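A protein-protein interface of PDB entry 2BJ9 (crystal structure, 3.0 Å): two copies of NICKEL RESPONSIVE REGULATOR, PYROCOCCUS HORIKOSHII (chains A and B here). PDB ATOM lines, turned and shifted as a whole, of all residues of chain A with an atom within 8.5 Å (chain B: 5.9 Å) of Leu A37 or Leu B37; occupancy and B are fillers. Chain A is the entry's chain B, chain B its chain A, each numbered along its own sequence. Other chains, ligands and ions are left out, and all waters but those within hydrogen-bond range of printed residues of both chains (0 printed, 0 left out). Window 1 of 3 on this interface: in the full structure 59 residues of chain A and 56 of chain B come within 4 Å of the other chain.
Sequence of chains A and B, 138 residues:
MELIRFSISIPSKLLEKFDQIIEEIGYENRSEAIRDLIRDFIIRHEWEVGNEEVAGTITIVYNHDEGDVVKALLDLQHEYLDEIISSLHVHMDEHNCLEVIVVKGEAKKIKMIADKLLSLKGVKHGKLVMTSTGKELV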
ATOM      1  N   ILE A  10      22.026 -36.866 -30.277  1.00  0.00           N
ATOM      2  CA  ILE A  10      22.814 -36.146 -31.268  1.00  0.00           C
ATOM      3  C   ILE A  10      23.011 -36.968 -32.549  1.00  0.00           C
ATOM      4  O   ILE A  10      23.075 -38.195 -32.505  1.00  0.00           O
ATOM      5  CB  ILE A  10      24.203 -35.813 -30.681  1.00  0.00           C
ATOM      6  CG1 ILE A  10      24.034 -34.920 -29.454  1.00  0.00           C
ATOM      7  CG2 ILE A  10      25.095 -35.162 -31.732  1.00  0.00           C
ATOM      8  CD1 ILE A  10      23.350 -33.611 -29.743  1.00  0.00           C
ATOM      9  N   LEU A  14      27.672 -36.505 -36.600  1.00  0.00           N
ATOM     10  CA  LEU A  14      28.088 -35.255 -35.993  1.00  0.00           C
ATOM     11  C   LEU A  14      28.845 -35.612 -34.719  1.00  0.00           C
ATOM     12  O   LEU A  14      29.925 -35.095 -34.460  1.00  0.00           O
ATOM     13  CB  LEU A  14      26.860 -34.412 -35.656  1.00  0.00           C
ATOM     14  CG  LEU A  14      27.073 -33.077 -34.957  1.00  0.00           C
ATOM     15  CD1 LEU A  14      27.778 -32.119 -35.897  1.00  0.00           C
ATOM     16  CD2 LEU A  14      25.726 -32.521 -34.525  1.00  0.00           C
ATOM     17  N   PHE A  18      32.675 -35.003 -33.562  1.00  0.00           N
ATOM     18  CA  PHE A  18      32.943 -34.274 -32.327  1.00  0.00           C
ATOM     19  C   PHE A  18      33.959 -35.059 -31.515  1.00  0.00           C
ATOM     20  O   PHE A  18      35.033 -34.558 -31.201  1.00  0.00           O
ATOM     21  CB  PHE A  18      31.651 -34.112 -31.525  1.00  0.00           C
ATOM     22  CG  PHE A  18      31.809 -33.317 -30.256  1.00  0.00           C
ATOM     23  CD1 PHE A  18      32.336 -32.033 -30.281  1.00  0.00           C
ATOM     24  CD2 PHE A  18      31.403 -33.848 -29.038  1.00  0.00           C
ATOM     25  CE1 PHE A  18      32.456 -31.294 -29.114  1.00  0.00           C
ATOM     26  CE2 PHE A  18      31.518 -33.116 -27.864  1.00  0.00           C
ATOM     27  CZ  PHE A  18      32.045 -31.835 -27.901  1.00  0.00           C
ATOM     28  N   ILE A  22      37.653 -33.689 -30.154  1.00  0.00           N
ATOM     29  CA  ILE A  22      38.038 -33.458 -28.764  1.00  0.00           C
ATOM     30  C   ILE A  22      39.230 -34.318 -28.346  1.00  0.00           C
ATOM     31  O   ILE A  22      39.923 -34.001 -27.380  1.00  0.00           O
ATOM     32  CB  ILE A  22      36.874 -33.713 -27.776  1.00  0.00           C
ATOM     33  CG1 ILE A  22      36.514 -35.188 -27.746  1.00  0.00           C
ATOM     34  CG2 ILE A  22      35.670 -32.891 -28.167  1.00  0.00           C
ATOM     35  CD1 ILE A  22      35.424 -35.491 -26.766  1.00  0.00           C
ATOM     36  N   TYR A  27      40.757 -33.064 -24.888  1.00  0.00           N
ATOM     37  CA  TYR A  27      39.769 -33.206 -23.824  1.00  0.00           C
ATOM     38  C   TYR A  27      39.820 -34.647 -23.371  1.00  0.00           C
ATOM     39  O   TYR A  27      40.028 -35.548 -24.180  1.00  0.00           O
ATOM     40  CB  TYR A  27      38.357 -32.884 -24.308  1.00  0.00           C
ATOM     41  CG  TYR A  27      38.080 -31.414 -24.520  1.00  0.00           C
ATOM     42  CD1 TYR A  27      38.524 -30.758 -25.665  1.00  0.00           C
ATOM     43  CD2 TYR A  27      37.362 -30.681 -23.577  1.00  0.00           C
ATOM     44  CE1 TYR A  27      38.256 -29.408 -25.867  1.00  0.00           C
ATOM     45  CE2 TYR A  27      37.090 -29.333 -23.769  1.00  0.00           C
ATOM     46  CZ  TYR A  27      37.538 -28.703 -24.915  1.00  0.00           C
ATOM     47  OH  TYR A  27      37.266 -27.372 -25.111  1.00  0.00           O
ATOM     48  N   ARG A  30      33.976 -36.325 -23.187  1.00  0.00           N
ATOM     49  CA  ARG A  30      33.010 -35.588 -23.975  1.00  0.00           C
ATOM     50  C   ARG A  30      32.184 -34.697 -23.053  1.00  0.00           C
ATOM     51  O   ARG A  30      31.807 -33.582 -23.427  1.00  0.00           O
ATOM     52  CB  ARG A  30      32.111 -36.577 -24.708  1.00  0.00           C
ATOM     53  CG  ARG A  30      30.929 -35.980 -25.436  1.00  0.00           C
ATOM     54  CD  ARG A  30      29.925 -37.082 -25.730  1.00  0.00           C
ATOM     55  NE  ARG A  30      30.501 -38.117 -26.578  1.00  0.00           N
ATOM     56  CZ  ARG A  30      30.057 -39.366 -26.644  1.00  0.00           C
ATOM     57  NH1 ARG A  30      29.028 -39.747 -25.905  1.00  0.00           N
ATOM     58  NH2 ARG A  30      30.641 -40.234 -27.456  1.00  0.00           N
ATOM     59  N   SER A  31      31.899 -35.183 -21.848  1.00  0.00           N
ATOM     60  CA  SER A  31      31.116 -34.388 -20.917  1.00  0.00           C
ATOM     61  C   SER A  31      31.781 -33.040 -20.714  1.00  0.00           C
ATOM     62  O   SER A  31      31.160 -31.995 -20.906  1.00  0.00           O
ATOM     63  CB  SER A  31      30.977 -35.105 -19.581  1.00  0.00           C
ATOM     64  OG  SER A  31      30.085 -36.200 -19.682  1.00  0.00           O
ATOM     65  N   GLU A  32      33.053 -33.061 -20.339  1.00  0.00           N
ATOM     66  CA  GLU A  32      33.782 -31.826 -20.120  1.00  0.00           C
ATOM     67  C   GLU A  32      33.600 -30.899 -21.311  1.00  0.00           C
ATOM     68  O   GLU A  32      33.176 -29.757 -21.159  1.00  0.00           O
ATOM     69  CB  GLU A  32      35.273 -32.104 -19.908  1.00  0.00           C
ATOM     70  CG  GLU A  32      36.142 -30.835 -19.922  1.00  0.00           C
ATOM     71  CD  GLU A  32      35.850 -29.890 -18.759  1.00  0.00           C
ATOM     72  OE1 GLU A  32      36.214 -28.693 -18.853  1.00  0.00           O
ATOM     73  OE2 GLU A  32      35.266 -30.348 -17.748  1.00  0.00           O
ATOM     74  N   ALA A  33      33.906 -31.396 -22.499  1.00  0.00           N
ATOM     75  CA  ALA A  33      33.784 -30.578 -23.692  1.00  0.00           C
ATOM     76  C   ALA A  33      32.396 -29.969 -23.834  1.00  0.00           C
ATOM     77  O   ALA A  33      32.261 -28.785 -24.132  1.00  0.00           O
ATOM     78  CB  ALA A  33      34.130 -31.395 -24.916  1.00  0.00           C
ATOM     79  N   ILE A  34      31.360 -30.773 -23.614  1.00  0.00           N
ATOM     80  CA  ILE A  34      29.997 -30.270 -23.738  1.00  0.00           C
ATOM     81  C   ILE A  34      29.684 -29.238 -22.664  1.00  0.00           C
ATOM     82  O   ILE A  34      28.974 -28.274 -22.930  1.00  0.00           O
ATOM     83  CB  ILE A  34      28.969 -31.416 -23.692  1.00  0.00           C
ATOM     84  CG1 ILE A  34      29.095 -32.254 -24.961  1.00  0.00           C
ATOM     85  CG2 ILE A  34      27.558 -30.863 -23.597  1.00  0.00           C
ATOM     86  CD1 ILE A  34      28.058 -33.312 -25.082  1.00  0.00           C
ATOM     87  N   ARG A  35      30.202 -29.431 -21.453  1.00  0.00           N
ATOM     88  CA  ARG A  35      29.975 -28.444 -20.407  1.00  0.00           C
ATOM     89  C   ARG A  35      30.629 -27.125 -20.830  1.00  0.00           C
ATOM     90  O   ARG A  35      30.027 -26.060 -20.711  1.00  0.00           O
ATOM     91  CB  ARG A  35      30.515 -28.930 -19.064  1.00  0.00           C
ATOM     92  CG  ARG A  35      29.424 -29.600 -18.231  1.00  0.00           C
ATOM     93  CD  ARG A  35      29.939 -30.185 -16.931  1.00  0.00           C
ATOM     94  NE  ARG A  35      30.227 -31.612 -17.042  1.00  0.00           N
ATOM     95  CZ  ARG A  35      31.431 -32.151 -16.867  1.00  0.00           C
ATOM     96  NH1 ARG A  35      32.470 -31.377 -16.575  1.00  0.00           N
ATOM     97  NH2 ARG A  35      31.594 -33.465 -16.974  1.00  0.00           N
ATOM     98  N   ASP A  36      31.848 -27.198 -21.353  1.00  0.00           N
ATOM     99  CA  ASP A  36      32.525 -26.004 -21.837  1.00  0.00           C
ATOM    100  C   ASP A  36      31.676 -25.306 -22.903  1.00  0.00           C
ATOM    101  O   ASP A  36      31.540 -24.082 -22.885  1.00  0.00           O
ATOM    102  CB  ASP A  36      33.890 -26.360 -22.424  1.00  0.00           C
ATOM    103  CG  ASP A  36      34.960 -26.522 -21.356  1.00  0.00           C
ATOM    104  OD1 ASP A  36      36.124 -26.780 -21.720  1.00  0.00           O
ATOM    105  OD2 ASP A  36      34.630 -26.390 -20.156  1.00  0.00           O
ATOM    106  N   LEU A  37      31.108 -26.076 -23.829  1.00  0.00           N
ATOM    107  CA  LEU A  37      30.261 -25.501 -24.876  1.00  0.00           C
ATOM    108  C   LEU A  37      29.118 -24.740 -24.226  1.00  0.00           C
ATOM    109  O   LEU A  37      28.876 -23.578 -24.540  1.00  0.00           O
ATOM    110  CB  LEU A  37      29.666 -26.585 -25.780  1.00  0.00           C
ATOM    111  CG  LEU A  37      30.611 -27.455 -26.598  1.00  0.00           C
ATOM    112  CD1 LEU A  37      29.788 -28.370 -27.483  1.00  0.00           C
ATOM    113  CD2 LEU A  37      31.529 -26.592 -27.434  1.00  0.00           C
ATOM    114  N   ILE A  38      28.410 -25.406 -23.321  1.00  0.00           N
ATOM    115  CA  ILE A  38      27.294 -24.778 -22.627  1.00  0.00           C
ATOM    116  C   ILE A  38      27.785 -23.533 -21.889  1.00  0.00           C
ATOM    117  O   ILE A  38      27.189 -22.461 -22.008  1.00  0.00           O
ATOM    118  CB  ILE A  38      26.633 -25.752 -21.620  1.00  0.00           C
ATOM    119  CG1 ILE A  38      26.064 -26.961 -22.368  1.00  0.00           C
ATOM    120  CG2 ILE A  38      25.518 -25.046 -20.875  1.00  0.00           C
ATOM    121  CD1 ILE A  38      25.390 -27.974 -21.485  1.00  0.00           C
ATOM    122  N   ARG A  39      28.872 -23.669 -21.131  1.00  0.00           N
ATOM    123  CA  ARG A  39      29.413 -22.526 -20.415  1.00  0.00           C
ATOM    124  C   ARG A  39      29.667 -21.370 -21.391  1.00  0.00           C
ATOM    125  O   ARG A  39      29.289 -20.229 -21.131  1.00  0.00           O
ATOM    126  CB  ARG A  39      30.710 -22.902 -19.697  1.00  0.00           C
ATOM    127  CG  ARG A  39      30.521 -23.481 -18.308  1.00  0.00           C
ATOM    128  CD  ARG A  39      31.846 -23.539 -17.555  1.00  0.00           C
ATOM    129  NE  ARG A  39      32.678 -24.637 -18.024  1.00  0.00           N
ATOM    130  CZ  ARG A  39      32.472 -25.904 -17.694  1.00  0.00           C
ATOM    131  NH1 ARG A  39      31.466 -26.220 -16.892  1.00  0.00           N
ATOM    132  NH2 ARG A  39      33.259 -26.852 -18.178  1.00  0.00           N
ATOM    133  N   ASP A  40      30.306 -21.670 -22.517  1.00  0.00           N
ATOM    134  CA  ASP A  40      30.586 -20.653 -23.515  1.00  0.00           C
ATOM    135  C   ASP A  40      29.284 -20.044 -24.022  1.00  0.00           C
ATOM    136  O   ASP A  40      29.172 -18.834 -24.191  1.00  0.00           O
ATOM    137  CB  ASP A  40      31.329 -21.268 -24.689  1.00  0.00           C
ATOM    138  CG  ASP A  40      31.555 -20.282 -25.810  1.00  0.00           C
ATOM    139  OD1 ASP A  40      32.279 -19.292 -25.585  1.00  0.00           O
ATOM    140  OD2 ASP A  40      31.007 -20.489 -26.914  1.00  0.00           O
ATOM    141  N   PHE A  41      28.302 -20.903 -24.268  1.00  0.00           N
ATOM    142  CA  PHE A  41      26.997 -20.487 -24.768  1.00  0.00           C
ATOM    143  C   PHE A  41      26.340 -19.493 -23.822  1.00  0.00           C
ATOM    144  O   PHE A  41      25.798 -18.473 -24.250  1.00  0.00           O
ATOM    145  CB  PHE A  41      26.114 -21.726 -24.956  1.00  0.00           C
ATOM    146  CG  PHE A  41      24.706 -21.415 -25.342  1.00  0.00           C
ATOM    147  CD1 PHE A  41      23.683 -21.489 -24.403  1.00  0.00           C
ATOM    148  CD2 PHE A  41      24.396 -21.039 -26.639  1.00  0.00           C
ATOM    149  CE1 PHE A  41      22.367 -21.190 -24.755  1.00  0.00           C
ATOM    150  CE2 PHE A  41      23.079 -20.736 -27.003  1.00  0.00           C
ATOM    151  CZ  PHE A  41      22.065 -20.813 -26.061  1.00  0.00           C
ATOM    152  N   ILE A  42      26.394 -19.805 -22.535  1.00  0.00           N
ATOM    153  CA  ILE A  42      25.825 -18.947 -21.509  1.00  0.00           C
ATOM    154  C   ILE A  42      26.577 -17.622 -21.462  1.00  0.00           C
ATOM    155  O   ILE A  42      25.973 -16.566 -21.292  1.00  0.00           O
ATOM    156  CB  ILE A  42      25.921 -19.607 -20.134  1.00  0.00           C
ATOM    157  CG1 ILE A  42      24.885 -20.713 -20.016  1.00  0.00           C
ATOM    158  CG2 ILE A  42      25.723 -18.587 -19.057  1.00  0.00           C
ATOM    159  CD1 ILE A  42      25.090 -21.564 -18.809  1.00  0.00           C
ATOM    160  N   ILE A  43      27.896 -17.690 -21.611  1.00  0.00           N
ATOM    161  CA  ILE A  43      28.739 -16.504 -21.585  1.00  0.00           C
ATOM    162  C   ILE A  43      28.470 -15.567 -22.765  1.00  0.00           C
ATOM    163  O   ILE A  43      28.437 -14.354 -22.590  1.00  0.00           O
ATOM    164  CB  ILE A  43      30.217 -16.902 -21.548  1.00  0.00           C
ATOM    165  CG1 ILE A  43      30.548 -17.445 -20.165  1.00  0.00           C
ATOM    166  CG2 ILE A  43      31.100 -15.720 -21.856  1.00  0.00           C
ATOM    167  CD1 ILE A  43      31.924 -18.008 -20.048  1.00  0.00           C
ATOM    168  N   ARG A  44      28.282 -16.113 -23.963  1.00  0.00           N
ATOM    169  CA  ARG A  44      27.984 -15.259 -25.108  1.00  0.00           C
ATOM    170  C   ARG A  44      26.662 -14.542 -24.841  1.00  0.00           C
ATOM    171  O   ARG A  44      26.529 -13.346 -25.086  1.00  0.00           O
ATOM    172  CB  ARG A  44      27.857 -16.080 -26.390  1.00  0.00           C
ATOM    173  CG  ARG A  44      29.164 -16.384 -27.094  1.00  0.00           C
ATOM    174  CD  ARG A  44      28.914 -17.321 -28.260  1.00  0.00           C
ATOM    175  NE  ARG A  44      30.104 -17.517 -29.083  1.00  0.00           N
ATOM    176  CZ  ARG A  44      30.176 -18.378 -30.096  1.00  0.00           C
ATOM    177  NH1 ARG A  44      31.297 -18.493 -30.798  1.00  0.00           N
ATOM    178  NH2 ARG A  44      29.124 -19.131 -30.403  1.00  0.00           N
ATOM    179  N   PHE B  18      21.152 -22.561 -18.591  1.00  0.00           N
ATOM    180  CA  PHE B  18      21.166 -23.020 -19.972  1.00  0.00           C
ATOM    181  C   PHE B  18      19.742 -23.250 -20.434  1.00  0.00           C
ATOM    182  O   PHE B  18      19.407 -22.970 -21.584  1.00  0.00           O
ATOM    183  CB  PHE B  18      21.953 -24.322 -20.105  1.00  0.00           C
ATOM    184  CG  PHE B  18      21.909 -24.922 -21.486  1.00  0.00           C
ATOM    185  CD1 PHE B  18      22.537 -24.293 -22.556  1.00  0.00           C
ATOM    186  CD2 PHE B  18      21.228 -26.111 -21.720  1.00  0.00           C
ATOM    187  CE1 PHE B  18      22.487 -24.841 -23.842  1.00  0.00           C
ATOM    188  CE2 PHE B  18      21.172 -26.667 -22.997  1.00  0.00           C
ATOM    189  CZ  PHE B  18      21.802 -26.029 -24.060  1.00  0.00           C
ATOM    190  N   GLU B  32      18.513 -30.130 -29.578  1.00  0.00           N
ATOM    191  CA  GLU B  32      18.678 -29.259 -30.732  1.00  0.00           C
ATOM    192  C   GLU B  32      19.798 -28.275 -30.436  1.00  0.00           C
ATOM    193  O   GLU B  32      20.712 -28.084 -31.239  1.00  0.00           O
ATOM    194  CB  GLU B  32      17.400 -28.468 -31.005  1.00  0.00           C
ATOM    195  CG  GLU B  32      16.198 -29.288 -31.412  1.00  0.00           C
ATOM    196  CD  GLU B  32      15.052 -28.411 -31.868  1.00  0.00           C
ATOM    197  OE1 GLU B  32      14.556 -27.594 -31.059  1.00  0.00           O
ATOM    198  OE2 GLU B  32      14.651 -28.535 -33.043  1.00  0.00           O
ATOM    199  N   ALA B  33      19.705 -27.647 -29.269  1.00  0.00           N
ATOM    200  CA  ALA B  33      20.681 -26.661 -28.829  1.00  0.00           C
ATOM    201  C   ALA B  33      22.095 -27.228 -28.776  1.00  0.00           C
ATOM    202  O   ALA B  33      22.983 -26.756 -29.486  1.00  0.00           O
ATOM    203  CB  ALA B  33      20.278 -26.124 -27.471  1.00  0.00           C
ATOM    204  N   ILE B  34      22.301 -28.242 -27.940  1.00  0.00           N
ATOM    205  CA  ILE B  34      23.617 -28.850 -27.814  1.00  0.00           C
ATOM    206  C   ILE B  34      24.122 -29.297 -29.181  1.00  0.00           C
ATOM    207  O   ILE B  34      25.308 -29.184 -29.477  1.00  0.00           O
ATOM    208  CB  ILE B  34      23.586 -30.039 -26.843  1.00  0.00           C
ATOM    209  CG1 ILE B  34      23.243 -29.541 -25.438  1.00  0.00           C
ATOM    210  CG2 ILE B  34      24.931 -30.729 -26.819  1.00  0.00           C
ATOM    211  CD1 ILE B  34      22.964 -30.647 -24.442  1.00  0.00           C
ATOM    212  N   ARG B  35      23.218 -29.791 -30.019  1.00  0.00           N
ATOM    213  CA  ARG B  35      23.594 -30.215 -31.362  1.00  0.00           C
ATOM    214  C   ARG B  35      24.280 -29.056 -32.070  1.00  0.00           C
ATOM    215  O   ARG B  35      25.370 -29.208 -32.620  1.00  0.00           O
ATOM    216  CB  ARG B  35      22.362 -30.615 -32.168  1.00  0.00           C
ATOM    217  CG  ARG B  35      22.627 -30.802 -33.664  1.00  0.00           C
ATOM    218  CD  ARG B  35      21.340 -30.649 -34.458  1.00  0.00           C
ATOM    219  NE  ARG B  35      20.752 -29.327 -34.260  1.00  0.00           N
ATOM    220  CZ  ARG B  35      19.463 -29.045 -34.411  1.00  0.00           C
ATOM    221  NH1 ARG B  35      18.610 -29.993 -34.764  1.00  0.00           N
ATOM    222  NH2 ARG B  35      19.023 -27.816 -34.200  1.00  0.00           N
ATOM    223  N   ASP B  36      23.635 -27.896 -32.055  1.00  0.00           N
ATOM    224  CA  ASP B  36      24.194 -26.728 -32.710  1.00  0.00           C
ATOM    225  C   ASP B  36      25.543 -26.336 -32.113  1.00  0.00           C
ATOM    226  O   ASP B  36      26.503 -26.105 -32.849  1.00  0.00           O
ATOM    227  CB  ASP B  36      23.212 -25.556 -32.639  1.00  0.00           C
ATOM    228  CG  ASP B  36      21.917 -25.837 -33.385  1.00  0.00           C
ATOM    229  OD1 ASP B  36      21.933 -26.684 -34.306  1.00  0.00           O
ATOM    230  OD2 ASP B  36      20.889 -25.203 -33.070  1.00  0.00           O
ATOM    231  N   LEU B  37      25.624 -26.277 -30.784  1.00  0.00           N
ATOM    232  CA  LEU B  37      26.875 -25.916 -30.128  1.00  0.00           C
ATOM    233  C   LEU B  37      28.002 -26.795 -30.655  1.00  0.00           C
ATOM    234  O   LEU B  37      29.100 -26.319 -30.926  1.00  0.00           O
ATOM    235  CB  LEU B  37      26.766 -26.099 -28.612  1.00  0.00           C
ATOM    236  CG  LEU B  37      25.691 -25.325 -27.839  1.00  0.00           C
ATOM    237  CD1 LEU B  37      25.918 -25.561 -26.360  1.00  0.00           C
ATOM    238  CD2 LEU B  37      25.746 -23.843 -28.144  1.00  0.00           C
ATOM    239  N   ILE B  38      27.716 -28.085 -30.796  1.00  0.00           N
ATOM    240  CA  ILE B  38      28.695 -29.043 -31.287  1.00  0.00           C
ATOM    241  C   ILE B  38      29.007 -28.781 -32.748  1.00  0.00           C
ATOM    242  O   ILE B  38      30.150 -28.884 -33.175  1.00  0.00           O
ATOM    243  CB  ILE B  38      28.183 -30.491 -31.133  1.00  0.00           C
ATOM    244  CG1 ILE B  38      28.117 -30.862 -29.646  1.00  0.00           C
ATOM    245  CG2 ILE B  38      29.097 -31.452 -31.881  1.00  0.00           C
ATOM    246  CD1 ILE B  38      27.240 -32.067 -29.333  1.00  0.00           C
ATOM    247  N   ARG B  39      27.990 -28.446 -33.524  1.00  0.00           N
ATOM    248  CA  ARG B  39      28.208 -28.169 -34.934  1.00  0.00           C
ATOM    249  C   ARG B  39      29.171 -26.996 -35.076  1.00  0.00           C
ATOM    250  O   ARG B  39      30.188 -27.098 -35.755  1.00  0.00           O
ATOM    251  CB  ARG B  39      26.882 -27.855 -35.617  1.00  0.00           C
ATOM    252  CG  ARG B  39      27.000 -27.506 -37.078  1.00  0.00           C
ATOM    253  CD  ARG B  39      25.624 -27.517 -37.719  1.00  0.00           C
ATOM    254  NE  ARG B  39      24.638 -26.790 -36.924  1.00  0.00           N
ATOM    255  CZ  ARG B  39      24.686 -25.484 -36.671  1.00  0.00           C
ATOM    256  NH1 ARG B  39      25.677 -24.738 -37.150  1.00  0.00           N
ATOM    257  NH2 ARG B  39      23.740 -24.922 -35.932  1.00  0.00           N
ATOM    258  N   ASP B  40      28.855 -25.887 -34.413  1.00  0.00           N
ATOM    259  CA  ASP B  40      29.693 -24.689 -34.452  1.00  0.00           C
ATOM    260  C   ASP B  40      31.117 -24.971 -33.973  1.00  0.00           C
ATOM    261  O   ASP B  40      32.071 -24.400 -34.488  1.00  0.00           O
ATOM    262  CB  ASP B  40      29.078 -23.585 -33.587  1.00  0.00           C
ATOM    263  CG  ASP B  40      27.741 -23.091 -34.124  1.00  0.00           C
ATOM    264  OD1 ASP B  40      27.001 -22.437 -33.354  1.00  0.00           O
ATOM    265  OD2 ASP B  40      27.436 -23.345 -35.314  1.00  0.00           O
ATOM    266  N   PHE B  41      31.254 -25.848 -32.983  1.00  0.00           N
ATOM    267  CA  PHE B  41      32.559 -26.212 -32.437  1.00  0.00           C
ATOM    268  C   PHE B  41      33.377 -26.928 -33.494  1.00  0.00           C
ATOM    269  O   PHE B  41      34.496 -26.535 -33.794  1.00  0.00           O
ATOM    270  CB  PHE B  41      32.385 -27.135 -31.231  1.00  0.00           C
ATOM    271  CG  PHE B  41      33.679 -27.685 -30.687  1.00  0.00           C
ATOM    272  CD1 PHE B  41      34.503 -26.907 -29.884  1.00  0.00           C
ATOM    273  CD2 PHE B  41      34.059 -28.997 -30.955  1.00  0.00           C
ATOM    274  CE1 PHE B  41      35.684 -27.426 -29.352  1.00  0.00           C
ATOM    275  CE2 PHE B  41      35.238 -29.525 -30.428  1.00  0.00           C
ATOM    276  CZ  PHE B  41      36.051 -28.735 -29.623  1.00  0.00           C
ATOM    277  N   ILE B  42      32.803 -27.986 -34.054  1.00  0.00           N
ATOM    278  CA  ILE B  42      33.465 -28.772 -35.084  1.00  0.00           C
ATOM    279  C   ILE B  42      33.969 -27.900 -36.224  1.00  0.00           C
ATOM    280  O   ILE B  42      35.026 -28.168 -36.787  1.00  0.00           O
ATOM    281  CB  ILE B  42      32.510 -29.835 -35.661  1.00  0.00           C
ATOM    282  CG1 ILE B  42      32.212 -30.897 -34.599  1.00  0.00           C
ATOM    283  CG2 ILE B  42      33.122 -30.464 -36.908  1.00  0.00           C
ATOM    284  CD1 ILE B  42      31.158 -31.907 -35.013  1.00  0.00           C
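Hydrophobic or aromatic side chains of chain A that line the printed part of chain B: Ile A10, Leu A14, Phe A18, Leu A37, Ile A38 and Phe A41.
Printed residues of chain B that touch a printed residue of chain A: Phe B18, Arg B35, Leu B37, Ile B38, Phe B41 and Ile B42.
Along chain B the printed residues that touch a printed residue of chain A span positions 18 to 42.
Among the printed residues, no Asp or Glu carboxylate lies within 4 Å of a Lys or Arg side-chain nitrogen of the other chain.
Phe A18 touches Ile B38, and with the chains exchanged Ile A38 touches Phe B18.
Phe A18 touches Phe B41, and with the chains exchanged Phe A41 touches Phe B18.
Leu A37 touches Ile B38, and with the chains exchanged Ile A38 touches Leu B37.
Leu A37 touches Phe B41, and with the chains exchanged Phe A41 touches Leu B37.
12 positions are printed for both chains.
NE of Arg B35 is in salt-bridge range of OD1 of Asp B36 (2.9 Å).
NE of Arg B35 sits close to O of Glu B32, 3.3 Å away.
Of chain B, only Leu B37, Ile B38 and Phe B41 come within 4 Å of Leu A37.
Leu B37 touches just these residues of chain A: Leu A37, Ile A38 and Phe A41.
Of the printed residues of chain B, Phe A18 touches Ile B38, Phe B41 and Ile B42.
Printed residues of chain A within 4 Å of Ile B38: Phe A18 and Leu A37.
Printed residues of chain B within 4 Å of Phe A41: Phe B18 (3.5 Å) and Leu B37 (3.5 Å).
Of the printed residues of chain A, Phe B18 touches Ile A38 (3.5 Å) and Phe A41 (3.5 Å).
Glu B32 touches none of the printed residues of chain A.
Among the printed residues, pairs that only touch across the chains: Ile A10 with Arg B35, Leu A14 with Arg B35, Leu A14 with Ile B42, Phe A18 with Ile B38, Phe A18 with Phe B41, Phe A18 with Ile B42, Leu A37 with Leu B37, Leu A37 with Ile B38, Leu A37 with Phe B41, Ile A38 with Phe B18, Ile A38 with Leu B37, Phe A41 with Phe B18 and Phe A41 with Leu B37.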
